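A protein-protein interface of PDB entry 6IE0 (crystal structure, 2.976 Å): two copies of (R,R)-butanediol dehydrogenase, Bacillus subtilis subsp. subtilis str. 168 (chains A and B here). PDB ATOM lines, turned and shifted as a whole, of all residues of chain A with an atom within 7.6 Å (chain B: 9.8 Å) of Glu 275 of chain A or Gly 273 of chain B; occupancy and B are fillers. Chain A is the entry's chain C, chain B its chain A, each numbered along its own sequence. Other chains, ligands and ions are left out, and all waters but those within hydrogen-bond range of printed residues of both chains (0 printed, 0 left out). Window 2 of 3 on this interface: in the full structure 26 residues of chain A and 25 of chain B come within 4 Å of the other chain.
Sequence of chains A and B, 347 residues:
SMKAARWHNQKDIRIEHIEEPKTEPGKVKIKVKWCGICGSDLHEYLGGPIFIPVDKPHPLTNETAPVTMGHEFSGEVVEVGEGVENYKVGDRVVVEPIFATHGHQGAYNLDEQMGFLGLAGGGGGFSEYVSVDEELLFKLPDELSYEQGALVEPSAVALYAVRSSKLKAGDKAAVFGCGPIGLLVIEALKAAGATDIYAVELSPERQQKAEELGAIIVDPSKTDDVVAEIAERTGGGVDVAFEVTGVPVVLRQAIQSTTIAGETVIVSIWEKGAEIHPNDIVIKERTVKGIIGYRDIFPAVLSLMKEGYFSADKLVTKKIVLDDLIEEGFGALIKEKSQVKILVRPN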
ATOM      1  N   VAL A 247     -11.100 -14.697   8.667  1.00  0.00           N
ATOM      2  CA  VAL A 247     -10.500 -15.874   9.289  1.00  0.00           C
ATOM      3  C   VAL A 247     -10.062 -15.488  10.699  1.00  0.00           C
ATOM      4  O   VAL A 247      -9.381 -14.464  10.859  1.00  0.00           O
ATOM      5  CB  VAL A 247      -9.306 -16.398   8.471  1.00  0.00           C
ATOM      6  CG1 VAL A 247      -8.730 -17.655   9.106  1.00  0.00           C
ATOM      7  CG2 VAL A 247      -9.724 -16.659   7.033  1.00  0.00           C
ATOM      8  N   PRO A 248     -10.425 -16.260  11.729  1.00  0.00           N
ATOM      9  CA  PRO A 248     -10.057 -15.873  13.104  1.00  0.00           C
ATOM     10  C   PRO A 248      -8.569 -15.632  13.307  1.00  0.00           C
ATOM     11  O   PRO A 248      -8.192 -14.670  13.987  1.00  0.00           O
ATOM     12  CB  PRO A 248     -10.555 -17.061  13.937  1.00  0.00           C
ATOM     13  CG  PRO A 248     -11.692 -17.609  13.148  1.00  0.00           C
ATOM     14  CD  PRO A 248     -11.290 -17.454  11.707  1.00  0.00           C
ATOM     15  N   VAL A 249      -7.712 -16.480  12.733  1.00  0.00           N
ATOM     16  CA  VAL A 249      -6.273 -16.319  12.924  1.00  0.00           C
ATOM     17  C   VAL A 249      -5.794 -14.982  12.376  1.00  0.00           C
ATOM     18  O   VAL A 249      -4.883 -14.364  12.936  1.00  0.00           O
ATOM     19  CB  VAL A 249      -5.519 -17.496  12.271  1.00  0.00           C
ATOM     20  CG1 VAL A 249      -4.031 -17.417  12.584  1.00  0.00           C
ATOM     21  CG2 VAL A 249      -6.107 -18.823  12.735  1.00  0.00           C
ATOM     22  N   VAL A 250      -6.409 -14.501  11.296  1.00  0.00           N
ATOM     23  CA  VAL A 250      -5.954 -13.259  10.683  1.00  0.00           C
ATOM     24  C   VAL A 250      -6.388 -12.047  11.502  1.00  0.00           C
ATOM     25  O   VAL A 250      -5.658 -11.051  11.573  1.00  0.00           O
ATOM     26  CB  VAL A 250      -6.461 -13.175   9.233  1.00  0.00           C
ATOM     27  CG1 VAL A 250      -5.937 -11.924   8.552  1.00  0.00           C
ATOM     28  CG2 VAL A 250      -6.050 -14.418   8.458  1.00  0.00           C
ATOM     29  N   LEU A 251      -7.565 -12.102  12.133  1.00  0.00           N
ATOM     30  CA  LEU A 251      -7.977 -11.007  13.006  1.00  0.00           C
ATOM     31  C   LEU A 251      -6.983 -10.818  14.143  1.00  0.00           C
ATOM     32  O   LEU A 251      -6.694  -9.685  14.548  1.00  0.00           O
ATOM     33  CB  LEU A 251      -9.381 -11.261  13.555  1.00  0.00           C
ATOM     34  CG  LEU A 251      -9.967 -10.153  14.440  1.00  0.00           C
ATOM     35  CD1 LEU A 251      -9.977  -8.813  13.714  1.00  0.00           C
ATOM     36  CD2 LEU A 251     -11.366 -10.514  14.917  1.00  0.00           C
ATOM     37  N   ARG A 252      -6.446 -11.922  14.668  1.00  0.00           N
ATOM     38  CA  ARG A 252      -5.388 -11.828  15.666  1.00  0.00           C
ATOM     39  C   ARG A 252      -4.166 -11.118  15.099  1.00  0.00           C
ATOM     40  O   ARG A 252      -3.581 -10.247  15.756  1.00  0.00           O
ATOM     41  CB  ARG A 252      -5.014 -13.225  16.161  1.00  0.00           C
ATOM     42  CG  ARG A 252      -5.805 -13.703  17.363  1.00  0.00           C
ATOM     43  CD  ARG A 252      -5.307 -15.060  17.839  1.00  0.00           C
ATOM     44  NE  ARG A 252      -6.140 -16.151  17.340  1.00  0.00           N
ATOM     45  CZ  ARG A 252      -5.708 -17.122  16.542  1.00  0.00           C
ATOM     46  NH1 ARG A 252      -4.441 -17.147  16.146  1.00  0.00           N
ATOM     47  NH2 ARG A 252      -6.543 -18.070  16.140  1.00  0.00           N
ATOM     48  N   GLN A 253      -3.769 -11.472  13.875  1.00  0.00           N
ATOM     49  CA  GLN A 253      -2.592 -10.863  13.265  1.00  0.00           C
ATOM     50  C   GLN A 253      -2.804  -9.378  12.998  1.00  0.00           C
ATOM     51  O   GLN A 253      -1.892  -8.570  13.212  1.00  0.00           O
ATOM     52  CB  GLN A 253      -2.240 -11.591  11.968  1.00  0.00           C
ATOM     53  CG  GLN A 253      -2.155 -13.099  12.105  1.00  0.00           C
ATOM     54  CD  GLN A 253      -1.724 -13.774  10.822  1.00  0.00           C
ATOM     55  OE1 GLN A 253      -2.466 -13.800   9.842  1.00  0.00           O
ATOM     56  NE2 GLN A 253      -0.519 -14.327  10.822  1.00  0.00           N
ATOM     57  N   TRP A 270     -18.653 -12.009   9.328  1.00  0.00           N
ATOM     58  CA  TRP A 270     -18.413 -13.030  10.343  1.00  0.00           C
ATOM     59  C   TRP A 270     -19.721 -13.716  10.711  1.00  0.00           C
ATOM     60  O   TRP A 270     -20.687 -13.047  11.095  1.00  0.00           O
ATOM     61  CB  TRP A 270     -17.760 -12.414  11.583  1.00  0.00           C
ATOM     62  CG  TRP A 270     -16.396 -11.857  11.322  1.00  0.00           C
ATOM     63  CD1 TRP A 270     -16.095 -10.629  10.809  1.00  0.00           C
ATOM     64  CD2 TRP A 270     -15.145 -12.515  11.553  1.00  0.00           C
ATOM     65  NE1 TRP A 270     -14.731 -10.480  10.709  1.00  0.00           N
ATOM     66  CE2 TRP A 270     -14.126 -11.624  11.160  1.00  0.00           C
ATOM     67  CE3 TRP A 270     -14.788 -13.768  12.057  1.00  0.00           C
ATOM     68  CZ2 TRP A 270     -12.777 -11.948  11.257  1.00  0.00           C
ATOM     69  CZ3 TRP A 270     -13.448 -14.088  12.149  1.00  0.00           C
ATOM     70  CH2 TRP A 270     -12.459 -13.183  11.752  1.00  0.00           C
ATOM     71  N   LYS A 272     -19.423 -17.160  12.453  1.00  0.00           N
ATOM     72  CA  LYS A 272     -19.039 -17.893  13.648  1.00  0.00           C
ATOM     73  C   LYS A 272     -18.129 -17.026  14.506  1.00  0.00           C
ATOM     74  O   LYS A 272     -17.732 -15.923  14.119  1.00  0.00           O
ATOM     75  CB  LYS A 272     -18.337 -19.210  13.287  1.00  0.00           C
ATOM     76  CG  LYS A 272     -19.233 -20.249  12.630  1.00  0.00           C
ATOM     77  CD  LYS A 272     -19.532 -21.414  13.569  1.00  0.00           C
ATOM     78  CE  LYS A 272     -20.465 -21.007  14.705  1.00  0.00           C
ATOM     79  NZ  LYS A 272     -20.612 -22.080  15.727  1.00  0.00           N
ATOM     80  N   GLY A 273     -17.803 -17.537  15.686  1.00  0.00           N
ATOM     81  CA  GLY A 273     -16.916 -16.830  16.578  1.00  0.00           C
ATOM     82  C   GLY A 273     -15.491 -16.797  16.053  1.00  0.00           C
ATOM     83  O   GLY A 273     -15.157 -17.320  14.989  1.00  0.00           O
ATOM     84  N   ALA A 274     -14.627 -16.167  16.844  1.00  0.00           N
ATOM     85  CA  ALA A 274     -13.213 -16.069  16.514  1.00  0.00           C
ATOM     86  C   ALA A 274     -12.440 -15.857  17.803  1.00  0.00           C
ATOM     87  O   ALA A 274     -12.839 -15.034  18.635  1.00  0.00           O
ATOM     88  CB  ALA A 274     -12.951 -14.922  15.532  1.00  0.00           C
ATOM     89  N   GLU A 275     -11.345 -16.591  17.969  1.00  0.00           N
ATOM     90  CA  GLU A 275     -10.526 -16.475  19.166  1.00  0.00           C
ATOM     91  C   GLU A 275      -9.519 -15.348  18.976  1.00  0.00           C
ATOM     92  O   GLU A 275      -8.682 -15.399  18.069  1.00  0.00           O
ATOM     93  CB  GLU A 275      -9.816 -17.791  19.471  1.00  0.00           C
ATOM     94  CG  GLU A 275      -8.628 -17.642  20.408  1.00  0.00           C
ATOM     95  CD  GLU A 275      -8.445 -18.836  21.318  1.00  0.00           C
ATOM     96  OE1 GLU A 275      -7.298 -19.087  21.750  1.00  0.00           O
ATOM     97  OE2 GLU A 275      -9.448 -19.522  21.605  1.00  0.00           O
ATOM     98  N   ILE A 276      -9.611 -14.335  19.829  1.00  0.00           N
ATOM     99  CA  ILE A 276      -8.646 -13.249  19.867  1.00  0.00           C
ATOM    100  C   ILE A 276      -7.860 -13.356  21.167  1.00  0.00           C
ATOM    101  O   ILE A 276      -8.159 -14.172  22.039  1.00  0.00           O
ATOM    102  CB  ILE A 276      -9.319 -11.868  19.736  1.00  0.00           C
ATOM    103  CG1 ILE A 276     -10.243 -11.617  20.928  1.00  0.00           C
ATOM    104  CG2 ILE A 276     -10.090 -11.771  18.428  1.00  0.00           C
ATOM    105  CD1 ILE A 276     -10.605 -10.157  21.127  1.00  0.00           C
ATOM    106  N   HIS A 277      -6.831 -12.520  21.288  1.00  0.00           N
ATOM    107  CA  HIS A 277      -6.078 -12.381  22.530  1.00  0.00           C
ATOM    108  C   HIS A 277      -6.407 -11.024  23.136  1.00  0.00           C
ATOM    109  O   HIS A 277      -5.761 -10.020  22.800  1.00  0.00           O
ATOM    110  CB  HIS A 277      -4.574 -12.520  22.284  1.00  0.00           C
ATOM    111  CG  HIS A 277      -4.174 -13.835  21.690  1.00  0.00           C
ATOM    112  ND1 HIS A 277      -4.973 -14.956  21.751  1.00  0.00           N
ATOM    113  CD2 HIS A 277      -3.054 -14.208  21.026  1.00  0.00           C
ATOM    114  CE1 HIS A 277      -4.365 -15.962  21.149  1.00  0.00           C
ATOM    115  NE2 HIS A 277      -3.199 -15.534  20.699  1.00  0.00           N
ATOM    116  N   PRO A 278      -7.412 -10.928  24.012  1.00  0.00           N
ATOM    117  CA  PRO A 278      -7.738  -9.623  24.611  1.00  0.00           C
ATOM    118  C   PRO A 278      -6.540  -8.945  25.249  1.00  0.00           C
ATOM    119  O   PRO A 278      -6.509  -7.711  25.349  1.00  0.00           O
ATOM    120  CB  PRO A 278      -8.806  -9.979  25.653  1.00  0.00           C
ATOM    121  CG  PRO A 278      -9.441 -11.220  25.125  1.00  0.00           C
ATOM    122  CD  PRO A 278      -8.336 -11.988  24.452  1.00  0.00           C
ATOM    123  N   ASN A 279      -5.544  -9.726  25.672  1.00  0.00           N
ATOM    124  CA  ASN A 279      -4.304  -9.153  26.182  1.00  0.00           C
ATOM    125  C   ASN A 279      -3.621  -8.292  25.125  1.00  0.00           C
ATOM    126  O   ASN A 279      -3.031  -7.254  25.447  1.00  0.00           O
ATOM    127  CB  ASN A 279      -3.375 -10.266  26.660  1.00  0.00           C
ATOM    128  CG  ASN A 279      -2.156  -9.735  27.382  1.00  0.00           C
ATOM    129  OD1 ASN A 279      -2.237  -9.329  28.543  1.00  0.00           O
ATOM    130  ND2 ASN A 279      -1.017  -9.737  26.700  1.00  0.00           N
ATOM    131  N   GLY B 246     -12.266 -10.771  33.120  1.00  0.00           N
ATOM    132  CA  GLY B 246     -11.293 -11.590  32.431  1.00  0.00           C
ATOM    133  C   GLY B 246     -11.841 -12.896  31.909  1.00  0.00           C
ATOM    134  O   GLY B 246     -11.059 -13.774  31.527  1.00  0.00           O
ATOM    135  N   VAL B 247     -13.155 -13.045  31.870  1.00  0.00           N
ATOM    136  CA  VAL B 247     -13.809 -14.278  31.435  1.00  0.00           C
ATOM    137  C   VAL B 247     -14.195 -14.132  29.967  1.00  0.00           C
ATOM    138  O   VAL B 247     -14.805 -13.122  29.598  1.00  0.00           O
ATOM    139  CB  VAL B 247     -15.050 -14.579  32.292  1.00  0.00           C
ATOM    140  CG1 VAL B 247     -15.729 -15.853  31.821  1.00  0.00           C
ATOM    141  CG2 VAL B 247     -14.670 -14.669  33.757  1.00  0.00           C
ATOM    142  N   PRO B 248     -13.838 -15.092  29.106  1.00  0.00           N
ATOM    143  CA  PRO B 248     -14.169 -14.955  27.677  1.00  0.00           C
ATOM    144  C   PRO B 248     -15.650 -14.753  27.411  1.00  0.00           C
ATOM    145  O   PRO B 248     -16.018 -13.907  26.588  1.00  0.00           O
ATOM    146  CB  PRO B 248     -13.657 -16.273  27.082  1.00  0.00           C
ATOM    147  CG  PRO B 248     -12.566 -16.702  28.020  1.00  0.00           C
ATOM    148  CD  PRO B 248     -13.042 -16.297  29.382  1.00  0.00           C
ATOM    149  N   VAL B 249     -16.515 -15.505  28.091  1.00  0.00           N
ATOM    150  CA  VAL B 249     -17.948 -15.356  27.867  1.00  0.00           C
ATOM    151  C   VAL B 249     -18.418 -13.964  28.261  1.00  0.00           C
ATOM    152  O   VAL B 249     -19.319 -13.401  27.627  1.00  0.00           O
ATOM    153  CB  VAL B 249     -18.724 -16.444  28.632  1.00  0.00           C
ATOM    154  CG1 VAL B 249     -20.122 -16.584  28.059  1.00  0.00           C
ATOM    155  CG2 VAL B 249     -17.970 -17.768  28.584  1.00  0.00           C
ATOM    156  N   LEU B 251     -16.617 -11.106  28.216  1.00  0.00           N
ATOM    157  CA  LEU B 251     -16.184 -10.124  27.225  1.00  0.00           C
ATOM    158  C   LEU B 251     -17.172 -10.058  26.065  1.00  0.00           C
ATOM    159  O   LEU B 251     -17.465  -8.974  25.547  1.00  0.00           O
ATOM    160  CB  LEU B 251     -14.782 -10.471  26.720  1.00  0.00           C
ATOM    161  CG  LEU B 251     -13.845  -9.412  26.103  1.00  0.00           C
ATOM    162  CD1 LEU B 251     -13.246  -9.917  24.807  1.00  0.00           C
ATOM    163  CD2 LEU B 251     -14.495  -8.048  25.883  1.00  0.00           C
ATOM    164  N   ARG B 252     -17.708 -11.211  25.658  1.00  0.00           N
ATOM    165  CA  ARG B 252     -18.747 -11.220  24.636  1.00  0.00           C
ATOM    166  C   ARG B 252     -19.979 -10.455  25.098  1.00  0.00           C
ATOM    167  O   ARG B 252     -20.553  -9.668  24.335  1.00  0.00           O
ATOM    168  CB  ARG B 252     -19.108 -12.659  24.273  1.00  0.00           C
ATOM    169  CG  ARG B 252     -18.267 -13.240  23.151  1.00  0.00           C
ATOM    170  CD  ARG B 252     -18.750 -14.625  22.757  1.00  0.00           C
ATOM    171  NE  ARG B 252     -17.998 -15.676  23.436  1.00  0.00           N
ATOM    172  CZ  ARG B 252     -18.540 -16.588  24.234  1.00  0.00           C
ATOM    173  NH1 ARG B 252     -19.849 -16.584  24.459  1.00  0.00           N
ATOM    174  NH2 ARG B 252     -17.773 -17.504  24.808  1.00  0.00           N
ATOM    175  N   ILE B 269      -7.092  -8.490  33.224  1.00  0.00           N
ATOM    176  CA  ILE B 269      -5.854  -9.133  32.792  1.00  0.00           C
ATOM    177  C   ILE B 269      -6.206 -10.451  32.119  1.00  0.00           C
ATOM    178  O   ILE B 269      -7.090 -11.181  32.585  1.00  0.00           O
ATOM    179  CB  ILE B 269      -4.897  -9.362  33.978  1.00  0.00           C
ATOM    180  CG1 ILE B 269      -4.668  -8.059  34.749  1.00  0.00           C
ATOM    181  CG2 ILE B 269      -3.578  -9.938  33.497  1.00  0.00           C
ATOM    182  CD1 ILE B 269      -5.417  -7.986  36.070  1.00  0.00           C
ATOM    183  N   TRP B 270      -5.515 -10.759  31.020  1.00  0.00           N
ATOM    184  CA  TRP B 270      -5.803 -11.937  30.208  1.00  0.00           C
ATOM    185  C   TRP B 270      -4.525 -12.728  29.973  1.00  0.00           C
ATOM    186  O   TRP B 270      -3.525 -12.170  29.511  1.00  0.00           O
ATOM    187  CB  TRP B 270      -6.430 -11.542  28.868  1.00  0.00           C
ATOM    188  CG  TRP B 270      -7.791 -10.938  29.011  1.00  0.00           C
ATOM    189  CD1 TRP B 270      -8.084  -9.655  29.369  1.00  0.00           C
ATOM    190  CD2 TRP B 270      -9.045 -11.596  28.807  1.00  0.00           C
ATOM    191  NE1 TRP B 270      -9.445  -9.472  29.399  1.00  0.00           N
ATOM    192  CE2 TRP B 270     -10.058 -10.648  29.056  1.00  0.00           C
ATOM    193  CE3 TRP B 270      -9.410 -12.893  28.436  1.00  0.00           C
ATOM    194  CZ2 TRP B 270     -11.412 -10.956  28.946  1.00  0.00           C
ATOM    195  CZ3 TRP B 270     -10.754 -13.198  28.330  1.00  0.00           C
ATOM    196  CH2 TRP B 270     -11.739 -12.233  28.580  1.00  0.00           C
ATOM    197  N   GLU B 271      -4.562 -14.024  30.289  1.00  0.00           N
ATOM    198  CA  GLU B 271      -3.440 -14.923  30.050  1.00  0.00           C
ATOM    199  C   GLU B 271      -3.665 -15.854  28.867  1.00  0.00           C
ATOM    200  O   GLU B 271      -2.716 -16.177  28.148  1.00  0.00           O
ATOM    201  CB  GLU B 271      -3.166 -15.776  31.293  1.00  0.00           C
ATOM    202  CG  GLU B 271      -2.574 -15.029  32.472  1.00  0.00           C
ATOM    203  CD  GLU B 271      -3.589 -14.785  33.571  1.00  0.00           C
ATOM    204  OE1 GLU B 271      -4.781 -15.100  33.364  1.00  0.00           O
ATOM    205  OE2 GLU B 271      -3.192 -14.292  34.649  1.00  0.00           O
ATOM    206  N   LYS B 272      -4.898 -16.296  28.655  1.00  0.00           N
ATOM    207  CA  LYS B 272      -5.259 -17.127  27.519  1.00  0.00           C
ATOM    208  C   LYS B 272      -6.118 -16.329  26.550  1.00  0.00           C
ATOM    209  O   LYS B 272      -6.510 -15.189  26.817  1.00  0.00           O
ATOM    210  CB  LYS B 272      -5.989 -18.393  27.984  1.00  0.00           C
ATOM    211  CG  LYS B 272      -5.161 -19.272  28.910  1.00  0.00           C
ATOM    212  CD  LYS B 272      -5.954 -20.475  29.401  1.00  0.00           C
ATOM    213  CE  LYS B 272      -6.128 -21.515  28.306  1.00  0.00           C
ATOM    214  NZ  LYS B 272      -5.134 -22.616  28.431  1.00  0.00           N
ATOM    215  N   GLY B 273      -6.409 -16.943  25.409  1.00  0.00           N
ATOM    216  CA  GLY B 273      -7.253 -16.319  24.418  1.00  0.00           C
ATOM    217  C   GLY B 273      -8.697 -16.239  24.880  1.00  0.00           C
ATOM    218  O   GLY B 273      -9.070 -16.647  25.980  1.00  0.00           O
ATOM    219  N   ALA B 274      -9.532 -15.702  23.996  1.00  0.00           N
ATOM    220  CA  ALA B 274     -10.957 -15.591  24.270  1.00  0.00           C
ATOM    221  C   ALA B 274     -11.702 -15.535  22.947  1.00  0.00           C
ATOM    222  O   ALA B 274     -11.307 -14.794  22.042  1.00  0.00           O
ATOM    223  CB  ALA B 274     -11.266 -14.348  25.109  1.00  0.00           C
ATOM    224  N   GLU B 275     -12.779 -16.307  22.846  1.00  0.00           N
ATOM    225  CA  GLU B 275     -13.593 -16.347  21.641  1.00  0.00           C
ATOM    226  C   GLU B 275     -14.634 -15.237  21.703  1.00  0.00           C
ATOM    227  O   GLU B 275     -15.461 -15.204  22.620  1.00  0.00           O
ATOM    228  CB  GLU B 275     -14.266 -17.709  21.490  1.00  0.00           C
ATOM    229  CG  GLU B 275     -15.402 -17.730  20.483  1.00  0.00           C
ATOM    230  CD  GLU B 275     -15.482 -19.041  19.729  1.00  0.00           C
ATOM    231  OE1 GLU B 275     -14.432 -19.701  19.568  1.00  0.00           O
ATOM    232  OE2 GLU B 275     -16.596 -19.413  19.301  1.00  0.00           O
ATOM    233  N   ILE B 276     -14.586 -14.331  20.733  1.00  0.00           N
ATOM    234  CA  ILE B 276     -15.589 -13.291  20.580  1.00  0.00           C
ATOM    235  C   ILE B 276     -16.403 -13.584  19.324  1.00  0.00           C
ATOM    236  O   ILE B 276     -16.091 -14.484  18.546  1.00  0.00           O
ATOM    237  CB  ILE B 276     -14.963 -11.883  20.513  1.00  0.00           C
ATOM    238  CG1 ILE B 276     -14.055 -11.765  19.284  1.00  0.00           C
ATOM    239  CG2 ILE B 276     -14.192 -11.577  21.781  1.00  0.00           C
ATOM    240  CD1 ILE B 276     -13.747 -10.340  18.884  1.00  0.00           C
ATOM    241  N   HIS B 277     -17.468 -12.806  19.132  1.00  0.00           N
ATOM    242  CA  HIS B 277     -18.248 -12.839  17.898  1.00  0.00           C
ATOM    243  C   HIS B 277     -17.986 -11.542  17.144  1.00  0.00           C
ATOM    244  O   HIS B 277     -18.682 -10.540  17.368  1.00  0.00           O
ATOM    245  CB  HIS B 277     -19.739 -13.021  18.187  1.00  0.00           C
ATOM    246  CG  HIS B 277     -20.055 -14.261  18.966  1.00  0.00           C
ATOM    247  ND1 HIS B 277     -19.169 -15.311  19.088  1.00  0.00           N
ATOM    248  CD2 HIS B 277     -21.160 -14.621  19.662  1.00  0.00           C
ATOM    249  CE1 HIS B 277     -19.714 -16.261  19.826  1.00  0.00           C
ATOM    250  NE2 HIS B 277     -20.921 -15.868  20.187  1.00  0.00           N
ATOM    251  N   PRO B 278     -16.983 -11.505  16.242  1.00  0.00           N
ATOM    252  CA  PRO B 278     -16.664 -10.266  15.516  1.00  0.00           C
ATOM    253  C   PRO B 278     -17.860  -9.641  14.814  1.00  0.00           C
ATOM    254  O   PRO B 278     -17.868  -8.436  14.548  1.00  0.00           O
ATOM    255  CB  PRO B 278     -15.602 -10.719  14.508  1.00  0.00           C
ATOM    256  CG  PRO B 278     -14.960 -11.890  15.152  1.00  0.00           C
ATOM    257  CD  PRO B 278     -16.058 -12.597  15.898  1.00  0.00           C
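Trp 270 of chain A touches Pro 278 of chain B, and with the chains exchanged Pro 278 of chain A touches Trp 270 of chain B.
Gly 273 of chain A touches Ile 276 of chain B, and with the chains exchanged Ile 276 of chain A touches Gly 273 of chain B.
Ala 274 of chain A touches Ile 276 of chain B, and with the chains exchanged Ile 276 of chain A touches Ala 274 of chain B.
Ile 276 of chain A touches its own counterpart, Ile 276 of chain B.
Of the printed residues of chain A, Gly 273 of chain B touches Glu 275, Ile 276 and His 277.
Ala 274 of chain A touches just these residues of chain B: Ala 274, Glu 275, Ile 276 and Pro 278.
Ile 276 of chain A touches three residues of chain B.
Printed residues of chain A within 4 Å of Glu 275 of chain B: Gly 273, Ala 274 and Glu 275.
Of the printed residues of chain A, Pro 278 of chain B touches Leu 251, Trp 270 and Ala 274.
Of the printed residues of chain A, Ala 274 of chain B touches Ala 274 (3.7 Å), Glu 275 (3.4 Å), Ile 276 (2.8 Å) and Pro 278 (3.6 Å).
Printed residues of chain B within 4 Å of Trp 270 of chain A: Pro 278.
Printed residues of chain B within 4 Å of Gly 273 of chain A: Glu 275 (3.8 Å), Ile 276 (3.2 Å) and His 277 (3.7 Å).
Lys 272 of chain B touches none of the printed residues of chain A.
Val 249 of chain B touches none of the printed residues of chain A.
The nearest residue of chain B that does not touch Glu 275 of chain A is Ile 276 of chain B (4.8 Å).
The nearest residue of chain A that does not touch Gly 273 of chain B is Pro 278 of chain A (4.3 Å).
The guanidinium group of Arg 252 of chain B lies within hydrogen-bond range of the backbone carbonyl oxygen of Glu 275 of chain B, 2.7 Å away.
The guanidinium group of Arg 252 of chain A lies within hydrogen-bond range of the backbone carbonyl oxygen of Glu 275 of chain A, 2.7 Å away.
The side-chain amide oxygen (OD1) of Asn 279 of chain A lies close to the backbone carbonyl oxygen (O) of Trp 270 of chain B (3.3 Å).
N of Ile 276 of chain A sits at hydrogen-bond distance from O of Ala 274 of chain B (2.8 Å).
The backbone carbonyl oxygen (O) of Ile 276 of chain B is in hydrogen-bond range of the backbone NH (N) of Ala 274 of chain A (2.8 Å).
Printed residues of chain A that touch a printed residue of chain B: Leu 251, Trp 270, Gly 273, Ala 274, Glu 275, Ile 276, His 277, Pro 278 and Asn 279.
Hydrophobic or aromatic side chains of chain A within 4 Å of the printed part of chain B: Leu 251, Trp 270, Ala 274, Ile 276, His 277 and Pro 278.
Of the 16 printed residues of chain B, 7 touch a printed residue of chain A.
Printed residues of chain B that touch a printed residue of chain A: Trp 270, Gly 273, Ala 274, Glu 275, Ile 276, His 277 and Pro 278.
Among the printed residues, pairs that only touch across the chains: Gly 273 of chain A with Ile 276 of chain B, Ile 276 of chain A with Gly 273 of chain B, Ala 274 of chain A with Glu 275 of chain B, Glu 275 of chain A with Ala 274 of chain B, Trp 270 of chain A with Pro 278 of chain B, Pro 278 of chain A with Trp 270 of chain B, Pro 278 of chain A with Ala 274 of chain B, Ala 274 of chain A with Pro 278 of chain B, Gly 273 of chain A with His 277 of chain B, Ala 274 of chain A with Ala 274 of chain B, His 277 of chain A with Gly 273 of chain B, Gly 273 of chain A with Glu 275 of chain B, Glu 275 of chain A with Gly 273 of chain B, Leu 251 of chain A with Pro 278 of chain B, Ile 276 of chain A with Ile 276 of chain B and Glu 275 of chain A with Glu 275 of chain B.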
